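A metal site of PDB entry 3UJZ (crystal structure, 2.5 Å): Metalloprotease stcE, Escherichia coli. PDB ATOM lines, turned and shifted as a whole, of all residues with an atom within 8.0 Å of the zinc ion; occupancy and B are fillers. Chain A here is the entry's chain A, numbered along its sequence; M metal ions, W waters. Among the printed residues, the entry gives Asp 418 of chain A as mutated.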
ATOM      1  N   HIS A 338      13.758  -5.217  35.473  1.00  0.00           N
ATOM      2  CA  HIS A 338      13.911  -6.534  36.079  1.00  0.00           C
ATOM      3  C   HIS A 338      14.568  -6.486  37.418  1.00  0.00           C
ATOM      4  O   HIS A 338      14.853  -7.558  37.971  1.00  0.00           O
ATOM      5  CB  HIS A 338      14.844  -7.405  35.189  1.00  0.00           C
ATOM      6  CG  HIS A 338      14.304  -7.816  33.856  1.00  0.00           C
ATOM      7  ND1 HIS A 338      12.944  -7.751  33.556  1.00  0.00           N
ATOM      8  CD2 HIS A 338      14.965  -8.287  32.770  1.00  0.00           C
ATOM      9  CE1 HIS A 338      12.839  -8.189  32.318  1.00  0.00           C
ATOM     10  NE2 HIS A 338      14.030  -8.510  31.800  1.00  0.00           N
ATOM     11  N   GLY A 398       8.181  -7.463  32.799  1.00  0.00           N
ATOM     12  CA  GLY A 398       8.850  -8.536  32.094  1.00  0.00           C
ATOM     13  C   GLY A 398       9.252  -9.798  32.848  1.00  0.00           C
ATOM     14  O   GLY A 398      10.243 -10.442  32.483  1.00  0.00           O
ATOM     15  N   SER A 399       8.486 -10.157  33.881  1.00  0.00           N
ATOM     16  CA  SER A 399       8.773 -11.398  34.616  1.00  0.00           C
ATOM     17  C   SER A 399       7.537 -12.106  35.246  1.00  0.00           C
ATOM     18  O   SER A 399       6.454 -11.512  35.332  1.00  0.00           O
ATOM     19  CB  SER A 399       9.961 -11.234  35.577  1.00  0.00           C
ATOM     20  OG  SER A 399       9.663 -10.512  36.749  1.00  0.00           O
ATOM     21  N   GLY A 400       7.732 -13.366  35.627  1.00  0.00           N
ATOM     22  CA  GLY A 400       6.701 -14.189  36.239  1.00  0.00           C
ATOM     23  C   GLY A 400       7.174 -15.603  36.508  1.00  0.00           C
ATOM     24  O   GLY A 400       8.050 -16.099  35.827  1.00  0.00           O
ATOM     25  N   GLU A 414       3.243  -9.277  26.527  1.00  0.00           N
ATOM     26  CA  GLU A 414       3.854  -9.234  27.860  1.00  0.00           C
ATOM     27  C   GLU A 414       3.003 -10.020  28.880  1.00  0.00           C
ATOM     28  O   GLU A 414       3.562 -10.814  29.627  1.00  0.00           O
ATOM     29  CB  GLU A 414       4.137  -7.805  28.317  1.00  0.00           C
ATOM     30  CG  GLU A 414       5.328  -7.799  29.247  1.00  0.00           C
ATOM     31  CD  GLU A 414       5.403  -6.703  30.272  1.00  0.00           C
ATOM     32  OE1 GLU A 414       5.512  -5.517  29.869  1.00  0.00           O
ATOM     33  OE2 GLU A 414       5.504  -7.036  31.469  1.00  0.00           O
ATOM     34  N   HIS A 417       3.130 -13.845  27.974  1.00  0.00           N
ATOM     35  CA  HIS A 417       4.483 -14.378  28.238  1.00  0.00           C
ATOM     36  C   HIS A 417       4.711 -14.534  29.752  1.00  0.00           C
ATOM     37  O   HIS A 417       4.865 -15.673  30.227  1.00  0.00           O
ATOM     38  CB  HIS A 417       5.567 -13.493  27.594  1.00  0.00           C
ATOM     39  CG  HIS A 417       6.983 -13.999  27.637  1.00  0.00           C
ATOM     40  ND1 HIS A 417       7.560 -14.651  26.549  1.00  0.00           N
ATOM     41  CD2 HIS A 417       7.947 -13.785  28.566  1.00  0.00           C
ATOM     42  CE1 HIS A 417       8.820 -14.878  26.902  1.00  0.00           C
ATOM     43  NE2 HIS A 417       9.116 -14.297  28.059  1.00  0.00           N
ATOM     44  N   ASP A 418       4.546 -13.417  30.505  1.00  0.00           N
ATOM     45  CA  ASP A 418       4.747 -13.382  31.947  1.00  0.00           C
ATOM     46  C   ASP A 418       3.932 -14.366  32.728  1.00  0.00           C
ATOM     47  O   ASP A 418       4.465 -15.015  33.629  1.00  0.00           O
ATOM     48  CB  ASP A 418       4.622 -11.938  32.492  1.00  0.00           C
ATOM     49  CG  ASP A 418       5.608 -10.959  31.845  1.00  0.00           C
ATOM     50  OD1 ASP A 418       6.624 -11.438  31.204  1.00  0.00           O
ATOM     51  OD2 ASP A 418       5.360  -9.732  31.927  1.00  0.00           O
ATOM     52  N   GLY A 420       2.562 -17.001  31.219  1.00  0.00           N
ATOM     53  CA  GLY A 420       2.981 -18.255  30.594  1.00  0.00           C
ATOM     54  C   GLY A 420       4.070 -18.916  31.413  1.00  0.00           C
ATOM     55  O   GLY A 420       4.017 -20.118  31.680  1.00  0.00           O
ATOM     56  N   HIS A 421       5.037 -18.091  31.858  1.00  0.00           N
ATOM     57  CA  HIS A 421       6.111 -18.500  32.746  1.00  0.00           C
ATOM     58  C   HIS A 421       5.604 -19.275  33.996  1.00  0.00           C
ATOM     59  O   HIS A 421       6.219 -20.271  34.369  1.00  0.00           O
ATOM     60  CB  HIS A 421       6.948 -17.296  33.147  1.00  0.00           C
ATOM     61  CG  HIS A 421       8.153 -17.079  32.263  1.00  0.00           C
ATOM     62  ND1 HIS A 421       9.006 -18.114  31.937  1.00  0.00           N
ATOM     63  CD2 HIS A 421       8.619 -15.935  31.716  1.00  0.00           C
ATOM     64  CE1 HIS A 421       9.960 -17.567  31.198  1.00  0.00           C
ATOM     65  NE2 HIS A 421       9.766 -16.267  31.033  1.00  0.00           N
ATOM     66  N   LEU A 425       6.340 -22.851  31.536  1.00  0.00           N
ATOM     67  CA  LEU A 425       6.923 -22.599  30.224  1.00  0.00           C
ATOM     68  C   LEU A 425       8.239 -21.806  30.301  1.00  0.00           C
ATOM     69  O   LEU A 425       8.439 -20.995  31.208  1.00  0.00           O
ATOM     70  CB  LEU A 425       5.911 -21.819  29.338  1.00  0.00           C
ATOM     71  CG  LEU A 425       4.563 -22.468  28.968  1.00  0.00           C
ATOM     72  CD1 LEU A 425       3.580 -21.420  28.543  1.00  0.00           C
ATOM     73  CD2 LEU A 425       4.725 -23.418  27.822  1.00  0.00           C
ATOM     74  N   GLY A 426       9.095 -22.029  29.322  1.00  0.00           N
ATOM     75  CA  GLY A 426      10.336 -21.298  29.145  1.00  0.00           C
ATOM     76  C   GLY A 426      10.237 -20.513  27.852  1.00  0.00           C
ATOM     77  O   GLY A 426       9.137 -20.292  27.311  1.00  0.00           O
ATOM     78  N   HIS A 427      11.369 -20.156  27.308  1.00  0.00           N
ATOM     79  CA  HIS A 427      11.391 -19.420  26.049  1.00  0.00           C
ATOM     80  C   HIS A 427      11.531 -20.340  24.900  1.00  0.00           C
ATOM     81  O   HIS A 427      12.243 -21.349  25.009  1.00  0.00           O
ATOM     82  CB  HIS A 427      12.544 -18.395  26.052  1.00  0.00           C
ATOM     83  CG  HIS A 427      12.421 -17.392  27.150  1.00  0.00           C
ATOM     84  ND1 HIS A 427      13.478 -16.605  27.507  1.00  0.00           N
ATOM     85  CD2 HIS A 427      11.366 -17.108  27.929  1.00  0.00           C
ATOM     86  CE1 HIS A 427      13.044 -15.866  28.505  1.00  0.00           C
ATOM     87  NE2 HIS A 427      11.796 -16.168  28.825  1.00  0.00           N
ATOM     88  N   TYR A 428      10.872 -19.997  23.769  1.00  0.00           N
ATOM     89  CA  TYR A 428      10.966 -20.731  22.508  1.00  0.00           C
ATOM     90  C   TYR A 428      10.763 -22.218  22.801  1.00  0.00           C
ATOM     91  O   TYR A 428      11.648 -23.039  22.600  1.00  0.00           O
ATOM     92  CB  TYR A 428      12.358 -20.418  21.846  1.00  0.00           C
ATOM     93  CG  TYR A 428      12.498 -18.950  21.497  1.00  0.00           C
ATOM     94  CD1 TYR A 428      11.852 -18.416  20.390  1.00  0.00           C
ATOM     95  CD2 TYR A 428      13.200 -18.084  22.314  1.00  0.00           C
ATOM     96  CE1 TYR A 428      11.926 -17.063  20.089  1.00  0.00           C
ATOM     97  CE2 TYR A 428      13.269 -16.713  22.034  1.00  0.00           C
ATOM     98  CZ  TYR A 428      12.619 -16.209  20.915  1.00  0.00           C
ATOM     99  OH  TYR A 428      12.645 -14.879  20.546  1.00  0.00           O
ATOM    100  N   ALA A 488       3.371 -17.309  22.153  1.00  0.00           N
ATOM    101  CA  ALA A 488       3.644 -16.237  23.026  1.00  0.00           C
ATOM    102  C   ALA A 488       4.848 -16.494  23.983  1.00  0.00           C
ATOM    103  O   ALA A 488       4.843 -16.001  25.067  1.00  0.00           O
ATOM    104  CB  ALA A 488       2.392 -15.902  23.788  1.00  0.00           C
ATOM    105  N   MET A 489       5.822 -17.309  23.615  1.00  0.00           N
ATOM    106  CA  MET A 489       7.060 -17.394  24.386  1.00  0.00           C
ATOM    107  C   MET A 489       8.156 -17.252  23.389  1.00  0.00           C
ATOM    108  O   MET A 489       9.299 -17.567  23.637  1.00  0.00           O
ATOM    109  CB  MET A 489       7.249 -18.698  25.163  1.00  0.00           C
ATOM    110  CG  MET A 489       6.157 -19.108  26.112  1.00  0.00           C
ATOM    111  SD  MET A 489       5.640 -18.004  27.535  1.00  0.00           S
ATOM    112  CE  MET A 489       7.211 -18.156  28.692  1.00  0.00           C
HETATM  113 ZN    ZN M   1      10.311 -14.879  29.685  1.00  0.00          ZN
HETATM  114  O   HOH W   1      11.363 -12.939  30.270  1.00  0.00           O
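ND1 of His 421 sits at hydrogen-bond distance from O of Leu 425, 3.0 Å away.
O of Ala 488 lies within hydrogen-bond range of ND1 of His 417 (3.4 Å).
Within 4 Å of the zinc ion: His 417, His 421 and His 427.
The zinc ion is bound by NE2 of His 421 (2.0 Å), NE2 of His 417 (2.1 Å), NE2 of His 427 (2.1 Å) and water W1 (2.3 Å).
The zinc ion has four donor atoms within binding distance.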
